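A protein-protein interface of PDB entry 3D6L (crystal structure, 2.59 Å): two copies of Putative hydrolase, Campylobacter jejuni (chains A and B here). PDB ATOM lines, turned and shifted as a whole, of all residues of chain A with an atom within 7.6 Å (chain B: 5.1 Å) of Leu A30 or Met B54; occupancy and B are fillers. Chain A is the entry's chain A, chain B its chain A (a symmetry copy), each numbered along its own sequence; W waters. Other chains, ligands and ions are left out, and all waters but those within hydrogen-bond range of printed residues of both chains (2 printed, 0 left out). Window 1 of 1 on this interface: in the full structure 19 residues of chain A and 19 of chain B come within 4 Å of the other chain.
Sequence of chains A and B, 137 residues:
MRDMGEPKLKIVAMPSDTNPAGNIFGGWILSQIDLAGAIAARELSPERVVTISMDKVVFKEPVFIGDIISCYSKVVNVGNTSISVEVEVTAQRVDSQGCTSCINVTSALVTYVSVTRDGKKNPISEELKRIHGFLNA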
ATOM      1  N   PHE A  25     -21.245   6.647  -8.609  1.00  0.00           N
ATOM      2  CA  PHE A  25     -20.022   7.374  -8.328  1.00  0.00           C
ATOM      3  C   PHE A  25     -19.414   7.948  -9.608  1.00  0.00           C
ATOM      4  O   PHE A  25     -19.260   7.240 -10.599  1.00  0.00           O
ATOM      5  CB  PHE A  25     -19.065   6.424  -7.586  1.00  0.00           C
ATOM      6  CG  PHE A  25     -17.705   6.989  -7.302  1.00  0.00           C
ATOM      7  CD1 PHE A  25     -16.569   6.214  -7.547  1.00  0.00           C
ATOM      8  CD2 PHE A  25     -17.547   8.272  -6.766  1.00  0.00           C
ATOM      9  CE1 PHE A  25     -15.286   6.708  -7.284  1.00  0.00           C
ATOM     10  CE2 PHE A  25     -16.268   8.783  -6.497  1.00  0.00           C
ATOM     11  CZ  PHE A  25     -15.136   7.998  -6.761  1.00  0.00           C
ATOM     12  N   GLY A  26     -19.092   9.240  -9.580  1.00  0.00           N
ATOM     13  CA  GLY A  26     -18.506   9.938 -10.725  1.00  0.00           C
ATOM     14  C   GLY A  26     -17.215   9.311 -11.219  1.00  0.00           C
ATOM     15  O   GLY A  26     -16.974   9.266 -12.423  1.00  0.00           O
ATOM     16  N   GLY A  27     -16.393   8.821 -10.292  1.00  0.00           N
ATOM     17  CA  GLY A  27     -15.149   8.111 -10.625  1.00  0.00           C
ATOM     18  C   GLY A  27     -15.336   6.819 -11.421  1.00  0.00           C
ATOM     19  O   GLY A  27     -14.492   6.473 -12.263  1.00  0.00           O
ATOM     20  N   TRP A  28     -16.424   6.099 -11.144  1.00  0.00           N
ATOM     21  CA  TRP A  28     -16.820   4.956 -11.961  1.00  0.00           C
ATOM     22  C   TRP A  28     -17.152   5.416 -13.384  1.00  0.00           C
ATOM     23  O   TRP A  28     -16.750   4.765 -14.345  1.00  0.00           O
ATOM     24  CB  TRP A  28     -18.005   4.215 -11.331  1.00  0.00           C
ATOM     25  CG  TRP A  28     -18.514   3.036 -12.131  1.00  0.00           C
ATOM     26  CD1 TRP A  28     -18.081   1.741 -12.048  1.00  0.00           C
ATOM     27  CD2 TRP A  28     -19.558   3.046 -13.126  1.00  0.00           C
ATOM     28  NE1 TRP A  28     -18.784   0.945 -12.930  1.00  0.00           N
ATOM     29  CE2 TRP A  28     -19.696   1.719 -13.601  1.00  0.00           C
ATOM     30  CE3 TRP A  28     -20.381   4.045 -13.664  1.00  0.00           C
ATOM     31  CZ2 TRP A  28     -20.627   1.366 -14.590  1.00  0.00           C
ATOM     32  CZ3 TRP A  28     -21.305   3.697 -14.645  1.00  0.00           C
ATOM     33  CH2 TRP A  28     -21.418   2.365 -15.100  1.00  0.00           C
ATOM     34  N   ILE A  29     -17.866   6.537 -13.520  1.00  0.00           N
ATOM     35  CA  ILE A  29     -18.207   7.053 -14.859  1.00  0.00           C
ATOM     36  C   ILE A  29     -16.950   7.435 -15.620  1.00  0.00           C
ATOM     37  O   ILE A  29     -16.764   7.053 -16.780  1.00  0.00           O
ATOM     38  CB  ILE A  29     -19.152   8.279 -14.837  1.00  0.00           C
ATOM     39  CG1 ILE A  29     -20.374   8.025 -13.953  1.00  0.00           C
ATOM     40  CG2 ILE A  29     -19.607   8.592 -16.252  1.00  0.00           C
ATOM     41  CD1 ILE A  29     -21.215   9.269 -13.714  1.00  0.00           C
ATOM     42  N   LEU A  30     -16.091   8.196 -14.956  1.00  0.00           N
ATOM     43  CA  LEU A  30     -14.814   8.616 -15.518  1.00  0.00           C
ATOM     44  C   LEU A  30     -13.936   7.451 -15.975  1.00  0.00           C
ATOM     45  O   LEU A  30     -13.149   7.601 -16.907  1.00  0.00           O
ATOM     46  CB  LEU A  30     -14.078   9.490 -14.501  1.00  0.00           C
ATOM     47  CG  LEU A  30     -14.053  11.002 -14.747  1.00  0.00           C
ATOM     48  CD1 LEU A  30     -15.232  11.482 -15.563  1.00  0.00           C
ATOM     49  CD2 LEU A  30     -14.010  11.737 -13.432  1.00  0.00           C
ATOM     50  N   SER A  31     -14.067   6.302 -15.306  1.00  0.00           N
ATOM     51  CA  SER A  31     -13.384   5.062 -15.702  1.00  0.00           C
ATOM     52  C   SER A  31     -13.909   4.587 -17.049  1.00  0.00           C
ATOM     53  O   SER A  31     -13.124   4.256 -17.951  1.00  0.00           O
ATOM     54  CB  SER A  31     -13.591   3.957 -14.662  1.00  0.00           C
ATOM     55  OG  SER A  31     -13.168   4.370 -13.375  1.00  0.00           O
ATOM     56  N   GLN A  32     -15.239   4.558 -17.175  1.00  0.00           N
ATOM     57  CA  GLN A  32     -15.899   4.228 -18.433  1.00  0.00           C
ATOM     58  C   GLN A  32     -15.472   5.165 -19.563  1.00  0.00           C
ATOM     59  O   GLN A  32     -15.245   4.724 -20.697  1.00  0.00           O
ATOM     60  CB  GLN A  32     -17.422   4.263 -18.280  1.00  0.00           C
ATOM     61  CG  GLN A  32     -17.979   3.541 -17.047  1.00  0.00           C
ATOM     62  CD  GLN A  32     -17.290   2.201 -16.721  1.00  0.00           C
ATOM     63  OE1 GLN A  32     -17.112   1.336 -17.591  1.00  0.00           O
ATOM     64  NE2 GLN A  32     -16.912   2.032 -15.447  1.00  0.00           N
ATOM     65  N   ILE A  33     -15.356   6.455 -19.242  1.00  0.00           N
ATOM     66  CA  ILE A  33     -14.958   7.473 -20.223  1.00  0.00           C
ATOM     67  C   ILE A  33     -13.531   7.228 -20.696  1.00  0.00           C
ATOM     68  O   ILE A  33     -13.268   7.200 -21.903  1.00  0.00           O
ATOM     69  CB  ILE A  33     -15.129   8.900 -19.658  1.00  0.00           C
ATOM     70  CG1 ILE A  33     -16.626   9.227 -19.543  1.00  0.00           C
ATOM     71  CG2 ILE A  33     -14.400   9.930 -20.518  1.00  0.00           C
ATOM     72  CD1 ILE A  33     -16.961  10.420 -18.662  1.00  0.00           C
ATOM     73  N   ASP A  34     -12.624   7.021 -19.745  1.00  0.00           N
ATOM     74  CA  ASP A  34     -11.228   6.778 -20.060  1.00  0.00           C
ATOM     75  C   ASP A  34     -11.074   5.548 -20.953  1.00  0.00           C
ATOM     76  O   ASP A  34     -10.361   5.588 -21.958  1.00  0.00           O
ATOM     77  CB  ASP A  34     -10.400   6.644 -18.779  1.00  0.00           C
ATOM     78  CG  ASP A  34      -8.902   6.780 -19.035  1.00  0.00           C
ATOM     79  OD1 ASP A  34      -8.510   7.155 -20.162  1.00  0.00           O
ATOM     80  OD2 ASP A  34      -8.104   6.518 -18.114  1.00  0.00           O
ATOM     81  N   LEU A  35     -11.772   4.469 -20.610  1.00  0.00           N
ATOM     82  CA  LEU A  35     -11.725   3.234 -21.399  1.00  0.00           C
ATOM     83  C   LEU A  35     -12.372   3.342 -22.789  1.00  0.00           C
ATOM     84  O   LEU A  35     -11.825   2.819 -23.770  1.00  0.00           O
ATOM     85  CB  LEU A  35     -12.341   2.076 -20.615  1.00  0.00           C
ATOM     86  CG  LEU A  35     -11.541   1.535 -19.429  1.00  0.00           C
ATOM     87  CD1 LEU A  35     -12.381   0.517 -18.653  1.00  0.00           C
ATOM     88  CD2 LEU A  35     -10.193   0.935 -19.861  1.00  0.00           C
ATOM     89  N   ALA A  36     -13.533   4.000 -22.864  1.00  0.00           N
ATOM     90  CA  ALA A  36     -14.258   4.190 -24.130  1.00  0.00           C
ATOM     91  C   ALA A  36     -13.482   5.075 -25.101  1.00  0.00           C
ATOM     92  O   ALA A  36     -13.442   4.795 -26.299  1.00  0.00           O
ATOM     93  CB  ALA A  36     -15.629   4.771 -23.879  1.00  0.00           C
ATOM     94  N   MET A  54      -7.296  15.107 -19.695  1.00  0.00           N
ATOM     95  CA  MET A  54      -8.745  15.215 -19.750  1.00  0.00           C
ATOM     96  C   MET A  54      -9.160  16.663 -19.575  1.00  0.00           C
ATOM     97  O   MET A  54      -8.758  17.319 -18.616  1.00  0.00           O
ATOM     98  CB  MET A  54      -9.399  14.411 -18.634  1.00  0.00           C
ATOM     99  CG  MET A  54      -9.578  12.961 -18.915  1.00  0.00           C
ATOM    100  SD  MET A  54     -11.068  12.350 -18.101  1.00  0.00           S
ATOM    101  CE  MET A  54     -10.951  10.613 -18.556  1.00  0.00           C
ATOM    102  N   ASP A  55      -9.984  17.147 -20.489  1.00  0.00           N
ATOM    103  CA  ASP A  55     -10.530  18.484 -20.402  1.00  0.00           C
ATOM    104  C   ASP A  55     -12.033  18.454 -20.549  1.00  0.00           C
ATOM    105  O   ASP A  55     -12.591  17.457 -20.989  1.00  0.00           O
ATOM    106  CB  ASP A  55      -9.940  19.346 -21.504  1.00  0.00           C
ATOM    107  CG  ASP A  55      -8.861  20.256 -20.997  1.00  0.00           C
ATOM    108  OD1 ASP A  55      -7.672  19.845 -21.074  1.00  0.00           O
ATOM    109  OD2 ASP A  55      -9.212  21.365 -20.493  1.00  0.00           O
ATOM    110  N   LYS A  56     -12.681  19.552 -20.176  1.00  0.00           N
ATOM    111  CA  LYS A  56     -14.096  19.778 -20.481  1.00  0.00           C
ATOM    112  C   LYS A  56     -14.998  18.586 -20.151  1.00  0.00           C
ATOM    113  O   LYS A  56     -15.882  18.220 -20.932  1.00  0.00           O
ATOM    114  CB  LYS A  56     -14.274  20.211 -21.951  1.00  0.00           C
ATOM    115  CG  LYS A  56     -13.465  21.453 -22.357  1.00  0.00           C
ATOM    116  CD  LYS A  56     -13.921  22.688 -21.581  1.00  0.00           C
ATOM    117  CE  LYS A  56     -12.879  23.804 -21.594  1.00  0.00           C
ATOM    118  NZ  LYS A  56     -13.214  24.818 -20.546  1.00  0.00           N
ATOM    119  N   VAL A  57     -14.758  17.966 -19.000  1.00  0.00           N
ATOM    120  CA  VAL A  57     -15.677  16.950 -18.518  1.00  0.00           C
ATOM    121  C   VAL A  57     -16.788  17.616 -17.731  1.00  0.00           C
ATOM    122  O   VAL A  57     -16.539  18.491 -16.899  1.00  0.00           O
ATOM    123  CB  VAL A  57     -14.978  15.756 -17.780  1.00  0.00           C
ATOM    124  CG1 VAL A  57     -13.475  15.962 -17.662  1.00  0.00           C
ATOM    125  CG2 VAL A  57     -15.661  15.405 -16.441  1.00  0.00           C
ATOM    126  N   VAL A  58     -18.020  17.237 -18.043  1.00  0.00           N
ATOM    127  CA  VAL A  58     -19.186  17.869 -17.455  1.00  0.00           C
ATOM    128  C   VAL A  58     -20.113  16.780 -16.960  1.00  0.00           C
ATOM    129  O   VAL A  58     -20.529  15.902 -17.723  1.00  0.00           O
ATOM    130  CB  VAL A  58     -19.939  18.798 -18.477  1.00  0.00           C
ATOM    131  CG1 VAL A  58     -21.160  19.479 -17.816  1.00  0.00           C
ATOM    132  CG2 VAL A  58     -18.988  19.843 -19.103  1.00  0.00           C
ATOM    133  N   PHE A  59     -20.417  16.823 -15.671  1.00  0.00           N
ATOM    134  CA  PHE A  59     -21.401  15.920 -15.091  1.00  0.00           C
ATOM    135  C   PHE A  59     -22.757  16.597 -15.206  1.00  0.00           C
ATOM    136  O   PHE A  59     -23.206  17.302 -14.297  1.00  0.00           O
ATOM    137  CB  PHE A  59     -21.036  15.580 -13.644  1.00  0.00           C
ATOM    138  CG  PHE A  59     -19.723  14.867 -13.515  1.00  0.00           C
ATOM    139  CD1 PHE A  59     -19.632  13.495 -13.767  1.00  0.00           C
ATOM    140  CD2 PHE A  59     -18.570  15.567 -13.166  1.00  0.00           C
ATOM    141  CE1 PHE A  59     -18.417  12.826 -13.667  1.00  0.00           C
ATOM    142  CE2 PHE A  59     -17.343  14.911 -13.063  1.00  0.00           C
ATOM    143  CZ  PHE A  59     -17.264  13.536 -13.313  1.00  0.00           C
ATOM    144  N   VAL A  89     -21.611  10.319 -22.696  1.00  0.00           N
ATOM    145  CA  VAL A  89     -22.224   9.224 -21.972  1.00  0.00           C
ATOM    146  C   VAL A  89     -23.736   9.438 -21.899  1.00  0.00           C
ATOM    147  O   VAL A  89     -24.197  10.533 -21.558  1.00  0.00           O
ATOM    148  CB  VAL A  89     -21.608   9.074 -20.558  1.00  0.00           C
ATOM    149  CG1 VAL A  89     -22.072   7.795 -19.903  1.00  0.00           C
ATOM    150  CG2 VAL A  89     -20.087   9.100 -20.630  1.00  0.00           C
ATOM    151  N   THR A 106     -23.147  12.566 -19.067  1.00  0.00           N
ATOM    152  CA  THR A 106     -21.822  13.163 -18.876  1.00  0.00           C
ATOM    153  C   THR A 106     -21.032  13.313 -20.188  1.00  0.00           C
ATOM    154  O   THR A 106     -21.351  12.692 -21.194  1.00  0.00           O
ATOM    155  CB  THR A 106     -20.980  12.518 -17.673  1.00  0.00           C
ATOM    156  OG1 THR A 106     -19.613  12.301 -18.057  1.00  0.00           O
ATOM    157  CG2 THR A 106     -21.556  11.224 -17.196  1.00  0.00           C
ATOM    158  N   SER A 107     -20.004  14.151 -20.146  1.00  0.00           N
ATOM    159  CA  SER A 107     -19.282  14.576 -21.329  1.00  0.00           C
ATOM    160  C   SER A 107     -17.802  14.766 -20.999  1.00  0.00           C
ATOM    161  O   SER A 107     -17.467  15.173 -19.892  1.00  0.00           O
ATOM    162  CB  SER A 107     -19.860  15.905 -21.776  1.00  0.00           C
ATOM    163  OG  SER A 107     -19.267  16.329 -22.970  1.00  0.00           O
ATOM    164  N   ALA A 108     -16.912  14.474 -21.942  1.00  0.00           N
ATOM    165  CA  ALA A 108     -15.480  14.680 -21.704  1.00  0.00           C
ATOM    166  C   ALA A 108     -14.648  14.745 -22.973  1.00  0.00           C
ATOM    167  O   ALA A 108     -15.007  14.169 -23.993  1.00  0.00           O
ATOM    168  CB  ALA A 108     -14.919  13.604 -20.757  1.00  0.00           C
ATOM    169  N   LEU A 109     -13.528  15.454 -22.880  1.00  0.00           N
ATOM    170  CA  LEU A 109     -12.534  15.526 -23.944  1.00  0.00           C
ATOM    171  C   LEU A 109     -11.248  14.903 -23.414  1.00  0.00           C
ATOM    172  O   LEU A 109     -10.591  15.481 -22.548  1.00  0.00           O
ATOM    173  CB  LEU A 109     -12.263  16.986 -24.312  1.00  0.00           C
ATOM    174  CG  LEU A 109     -12.074  17.440 -25.763  1.00  0.00           C
ATOM    175  CD1 LEU A 109     -11.347  18.797 -25.767  1.00  0.00           C
ATOM    176  CD2 LEU A 109     -11.354  16.412 -26.648  1.00  0.00           C
ATOM    177  N   VAL A 110     -10.890  13.731 -23.930  1.00  0.00           N
ATOM    178  CA  VAL A 110      -9.734  12.986 -23.423  1.00  0.00           C
ATOM    179  C   VAL A 110      -8.636  12.958 -24.479  1.00  0.00           C
ATOM    180  O   VAL A 110      -8.927  12.832 -25.671  1.00  0.00           O
ATOM    181  CB  VAL A 110     -10.114  11.509 -23.041  1.00  0.00           C
ATOM    182  CG1 VAL A 110      -9.087  10.921 -22.094  1.00  0.00           C
ATOM    183  CG2 VAL A 110     -11.510  11.428 -22.410  1.00  0.00           C
ATOM    184  N   TYR A 112      -4.940  11.077 -25.701  1.00  0.00           N
ATOM    185  CA  TYR A 112      -4.113   9.886 -25.599  1.00  0.00           C
ATOM    186  C   TYR A 112      -2.858  10.084 -26.431  1.00  0.00           C
ATOM    187  O   TYR A 112      -2.852  10.879 -27.373  1.00  0.00           O
ATOM    188  CB  TYR A 112      -4.890   8.654 -26.103  1.00  0.00           C
ATOM    189  CG  TYR A 112      -6.196   8.437 -25.372  1.00  0.00           C
ATOM    190  CD1 TYR A 112      -7.376   9.039 -25.810  1.00  0.00           C
ATOM    191  CD2 TYR A 112      -6.245   7.647 -24.224  1.00  0.00           C
ATOM    192  CE1 TYR A 112      -8.582   8.852 -25.123  1.00  0.00           C
ATOM    193  CE2 TYR A 112      -7.435   7.453 -23.528  1.00  0.00           C
ATOM    194  CZ  TYR A 112      -8.600   8.055 -23.977  1.00  0.00           C
ATOM    195  OH  TYR A 112      -9.771   7.863 -23.273  1.00  0.00           O
ATOM    196  N   GLY B  27      -8.580   5.682 -14.434  1.00  0.00           N
ATOM    197  CA  GLY B  27      -9.909   5.806 -13.817  1.00  0.00           C
ATOM    198  C   GLY B  27      -9.935   5.615 -12.301  1.00  0.00           C
ATOM    199  O   GLY B  27     -10.737   6.256 -11.600  1.00  0.00           O
ATOM    200  N   LEU B  30      -8.497   8.992 -11.076  1.00  0.00           N
ATOM    201  CA  LEU B  30      -9.573   9.967 -11.192  1.00  0.00           C
ATOM    202  C   LEU B  30     -10.638   9.833 -10.104  1.00  0.00           C
ATOM    203  O   LEU B  30     -11.260  10.822  -9.727  1.00  0.00           O
ATOM    204  CB  LEU B  30     -10.199   9.864 -12.585  1.00  0.00           C
ATOM    205  CG  LEU B  30      -9.850  10.953 -13.605  1.00  0.00           C
ATOM    206  CD1 LEU B  30      -8.508  11.599 -13.337  1.00  0.00           C
ATOM    207  CD2 LEU B  30      -9.869  10.380 -14.998  1.00  0.00           C
ATOM    208  N   ILE B  33      -9.129  11.448  -7.137  1.00  0.00           N
ATOM    209  CA  ILE B  33      -9.173  12.901  -7.359  1.00  0.00           C
ATOM    210  C   ILE B  33     -10.555  13.447  -7.032  1.00  0.00           C
ATOM    211  O   ILE B  33     -10.682  14.425  -6.287  1.00  0.00           O
ATOM    212  CB  ILE B  33      -8.743  13.267  -8.797  1.00  0.00           C
ATOM    213  CG1 ILE B  33      -7.234  13.027  -8.955  1.00  0.00           C
ATOM    214  CG2 ILE B  33      -9.117  14.706  -9.138  1.00  0.00           C
ATOM    215  CD1 ILE B  33      -6.736  12.975 -10.389  1.00  0.00           C
ATOM    216  N   ASP B  34     -11.587  12.796  -7.567  1.00  0.00           N
ATOM    217  CA  ASP B  34     -12.955  13.216  -7.337  1.00  0.00           C
ATOM    218  C   ASP B  34     -13.287  13.215  -5.845  1.00  0.00           C
ATOM    219  O   ASP B  34     -13.855  14.178  -5.329  1.00  0.00           O
ATOM    220  CB  ASP B  34     -13.930  12.334  -8.124  1.00  0.00           C
ATOM    221  CG  ASP B  34     -15.319  12.955  -8.237  1.00  0.00           C
ATOM    222  OD1 ASP B  34     -15.488  14.139  -7.867  1.00  0.00           O
ATOM    223  OD2 ASP B  34     -16.253  12.270  -8.697  1.00  0.00           O
ATOM    224  N   ILE B  52     -19.735  18.636 -10.489  1.00  0.00           N
ATOM    225  CA  ILE B  52     -20.344  19.131 -11.728  1.00  0.00           C
ATOM    226  C   ILE B  52     -19.402  19.161 -12.934  1.00  0.00           C
ATOM    227  O   ILE B  52     -19.855  19.024 -14.065  1.00  0.00           O
ATOM    228  CB  ILE B  52     -21.047  20.506 -11.558  1.00  0.00           C
ATOM    229  CG1 ILE B  52     -20.098  21.552 -10.962  1.00  0.00           C
ATOM    230  CG2 ILE B  52     -22.316  20.366 -10.723  1.00  0.00           C
ATOM    231  CD1 ILE B  52     -20.388  22.978 -11.441  1.00  0.00           C
ATOM    232  N   SER B  53     -18.103  19.343 -12.701  1.00  0.00           N
ATOM    233  CA  SER B  53     -17.147  19.344 -13.809  1.00  0.00           C
ATOM    234  C   SER B  53     -15.693  19.058 -13.424  1.00  0.00           C
ATOM    235  O   SER B  53     -15.317  19.104 -12.250  1.00  0.00           O
ATOM    236  CB  SER B  53     -17.245  20.649 -14.618  1.00  0.00           C
ATOM    237  OG  SER B  53     -16.831  21.764 -13.863  1.00  0.00           O
ATOM    238  N   MET B  54     -14.895  18.752 -14.447  1.00  0.00           N
ATOM    239  CA  MET B  54     -13.463  18.528 -14.335  1.00  0.00           C
ATOM    240  C   MET B  54     -12.751  19.152 -15.519  1.00  0.00           C
ATOM    241  O   MET B  54     -13.097  18.890 -16.668  1.00  0.00           O
ATOM    242  CB  MET B  54     -13.139  17.040 -14.337  1.00  0.00           C
ATOM    243  CG  MET B  54     -13.266  16.359 -13.019  1.00  0.00           C
ATOM    244  SD  MET B  54     -12.055  15.027 -12.888  1.00  0.00           S
ATOM    245  CE  MET B  54     -12.514  14.381 -11.274  1.00  0.00           C
ATOM    246  N   ASP B  55     -11.743  19.958 -15.232  1.00  0.00           N
ATOM    247  CA  ASP B  55     -10.917  20.554 -16.260  1.00  0.00           C
ATOM    248  C   ASP B  55      -9.455  20.306 -15.978  1.00  0.00           C
ATOM    249  O   ASP B  55      -9.093  19.930 -14.871  1.00  0.00           O
ATOM    250  CB  ASP B  55     -11.168  22.051 -16.307  1.00  0.00           C
ATOM    251  CG  ASP B  55     -12.060  22.444 -17.445  1.00  0.00           C
ATOM    252  OD1 ASP B  55     -13.295  22.532 -17.211  1.00  0.00           O
ATOM    253  OD2 ASP B  55     -11.524  22.629 -18.579  1.00  0.00           O
ATOM    254  N   LYS B  56      -8.618  20.519 -16.989  1.00  0.00           N
ATOM    255  CA  LYS B  56      -7.165  20.565 -16.816  1.00  0.00           C
ATOM    256  C   LYS B  56      -6.601  19.399 -15.999  1.00  0.00           C
ATOM    257  O   LYS B  56      -5.742  19.586 -15.130  1.00  0.00           O
ATOM    258  CB  LYS B  56      -6.730  21.918 -16.214  1.00  0.00           C
ATOM    259  CG  LYS B  56      -7.183  23.151 -17.013  1.00  0.00           C
ATOM    260  CD  LYS B  56      -6.546  23.175 -18.401  1.00  0.00           C
ATOM    261  CE  LYS B  56      -7.297  24.082 -19.372  1.00  0.00           C
ATOM    262  NZ  LYS B  56      -6.858  23.793 -20.772  1.00  0.00           N
ATOM    263  N   VAL B  57      -7.103  18.197 -16.262  1.00  0.00           N
ATOM    264  CA  VAL B  57      -6.500  17.013 -15.676  1.00  0.00           C
ATOM    265  C   VAL B  57      -5.360  16.544 -16.558  1.00  0.00           C
ATOM    266  O   VAL B  57      -5.494  16.475 -17.781  1.00  0.00           O
ATOM    267  CB  VAL B  57      -7.530  15.897 -15.290  1.00  0.00           C
ATOM    268  CG1 VAL B  57      -8.950  16.272 -15.688  1.00  0.00           C
ATOM    269  CG2 VAL B  57      -7.099  14.498 -15.776  1.00  0.00           C
ATOM    270  N   ALA B 108      -5.490  17.919 -11.486  1.00  0.00           N
ATOM    271  CA  ALA B 108      -6.855  18.184 -11.954  1.00  0.00           C
ATOM    272  C   ALA B 108      -7.504  19.394 -11.306  1.00  0.00           C
ATOM    273  O   ALA B 108      -7.175  19.760 -10.184  1.00  0.00           O
ATOM    274  CB  ALA B 108      -7.748  16.943 -11.775  1.00  0.00           C
ATOM    275  N   LEU B 109      -8.436  19.996 -12.037  1.00  0.00           N
ATOM    276  CA  LEU B 109      -9.262  21.090 -11.539  1.00  0.00           C
ATOM    277  C   LEU B 109     -10.706  20.606 -11.532  1.00  0.00           C
ATOM    278  O   LEU B 109     -11.307  20.428 -12.592  1.00  0.00           O
ATOM    279  CB  LEU B 109      -9.149  22.300 -12.471  1.00  0.00           C
ATOM    280  CG  LEU B 109      -9.067  23.733 -11.939  1.00  0.00           C
ATOM    281  CD1 LEU B 109      -9.460  24.705 -13.066  1.00  0.00           C
ATOM    282  CD2 LEU B 109      -9.900  23.976 -10.671  1.00  0.00           C
ATOM    283  N   VAL B 110     -11.263  20.394 -10.343  1.00  0.00           N
ATOM    284  CA  VAL B 110     -12.608  19.827 -10.210  1.00  0.00           C
ATOM    285  C   VAL B 110     -13.560  20.878  -9.653  1.00  0.00           C
ATOM    286  O   VAL B 110     -13.173  21.659  -8.780  1.00  0.00           O
ATOM    287  CB  VAL B 110     -12.621  18.572  -9.263  1.00  0.00           C
ATOM    288  CG1 VAL B 110     -13.853  17.726  -9.512  1.00  0.00           C
ATOM    289  CG2 VAL B 110     -11.360  17.716  -9.439  1.00  0.00           C
ATOM    290  N   THR B 111     -14.800  20.889 -10.134  1.00  0.00           N
ATOM    291  CA  THR B 111     -15.804  21.814  -9.611  1.00  0.00           C
ATOM    292  C   THR B 111     -16.999  21.075  -9.005  1.00  0.00           C
ATOM    293  O   THR B 111     -17.505  20.101  -9.572  1.00  0.00           O
ATOM    294  CB  THR B 111     -16.264  22.855 -10.676  1.00  0.00           C
ATOM    295  OG1 THR B 111     -15.114  23.430 -11.313  1.00  0.00           O
ATOM    296  CG2 THR B 111     -17.077  23.981 -10.033  1.00  0.00           C
HETATM  297  O   HOH W   1     -15.979  21.400 -17.745  1.00  0.00           O
HETATM  298  O   HOH W   2      -5.276  18.976 -19.566  1.00  0.00           O
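The backbone carbonyl oxygen of Asp A34 sits at hydrogen-bond distance from the side-chain hydroxyl of Tyr A112 (2.7 Å). The backbone NH (N) of Asp A55 lies within hydrogen-bond range of the backbone carbonyl oxygen (O) of Leu A109 (2.7 Å). The backbone NH (N) of Val A58 lies within hydrogen-bond range of the backbone carbonyl oxygen (O) of Ser A107 (2.8 Å). N of Ile B52 is in hydrogen-bond range of O of Thr B111 (2.8 Å). O of Ser B53 sits at hydrogen-bond distance from N of Thr B111 (2.8 Å). The backbone NH (N) of Asp B55 is in hydrogen-bond range of the backbone carbonyl oxygen (O) of Leu B109, 2.7 Å away.
Water W2 lies within hydrogen-bond range of OD1 of Asp A55 (3.0 Å) and O of Val B57 (3.1 Å). Water W1 lies within hydrogen-bond range of OD1 of Asp B55 (3.0 Å) and O of Val A57 (3.1 Å).
Hydrophobic or aromatic side chains of chain A within 4 Å of the printed part of chain B: Leu A30, Met A54, Val A57, Val A58 and Phe A59. Hydrophobic or aromatic side chains of chain B that line the printed part of chain A: Leu B30, Met B54 and Val B57.
Gly B27 touches its own counterpart, Gly A27. Leu A30 touches Met B54, and with the chains exchanged Met A54 touches Leu B30. Met A54 touches Val B57, and with the chains exchanged Val A57 touches Met B54. Asp A55 touches Lys B56, and with the chains exchanged Lys A56 touches Asp B55. 11 positions are printed for both chains. Of the 18 pairs that touch across the chains among the printed residues, 12 have their exchanged pair printed and touching as well.
CA of Gly A26 touches OD2 of Asp B34 (3.8 Å). Gly B27 touches Gly A27 (O to O, 3.8 Å). CE of Met B54 touches CD2 of Leu A30, 3.7 Å away. OG of Ser A31 touches O of Gly B27, at 3.6 Å. N of Gly B27 touches OD2 of Asp A34, 3.8 Å away. Leu B30 touches Met A54. Lys A56 touches Met B54 (N to O, 3.6 Å). CB of Ser B53 touches O of Val A57, 3.2 Å away. CA of Val A58 touches O of Ile B52, at 3.6 Å. Ser B53 touches Phe A59 (N to CD2, 3.8 Å).
N of Met A54 is in hydrogen-bond range of O of Val B57, at 3.0 Å. OD2 of Asp A55 is in salt-bridge range of NZ of Lys B56 (3.4 Å). The side-chain amino group (NZ) of Lys A56 is in salt-bridge range of the side-chain carboxylate (OD2) of Asp B55, 3.4 Å away. The backbone carbonyl oxygen (O) of Val A57 sits at hydrogen-bond distance from the backbone NH (N) of Met B54, at 3.0 Å. The backbone NH (N) of Phe A59 lies within hydrogen-bond range of the backbone carbonyl oxygen (O) of Ile B52, 2.8 Å away. The side-chain carboxylate of Asp A55 sits close to the side-chain carboxylate of Asp B55 (3.3 Å).
Of chain B, only Met B54 (3.7 Å) comes within 4 Å of Leu A30. Of chain A, only Leu A30 (3.7 Å), Lys A56 (3.6 Å) and Val A57 (3.0 Å) come within 4 Å of Met B54. Of the printed residues of chain A, Asp B34 touches Gly A26 and Gly A27. Of the printed residues of chain B, Gly A26 touches Asp B34 (3.8 Å). Printed residues of chain B within 4 Å of Lys A56: Met B54 (3.6 Å) and Asp B55 (3.4 Å). The nearest residue of chain B that does not touch Leu A30 is Leu B30 (4.2 Å).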
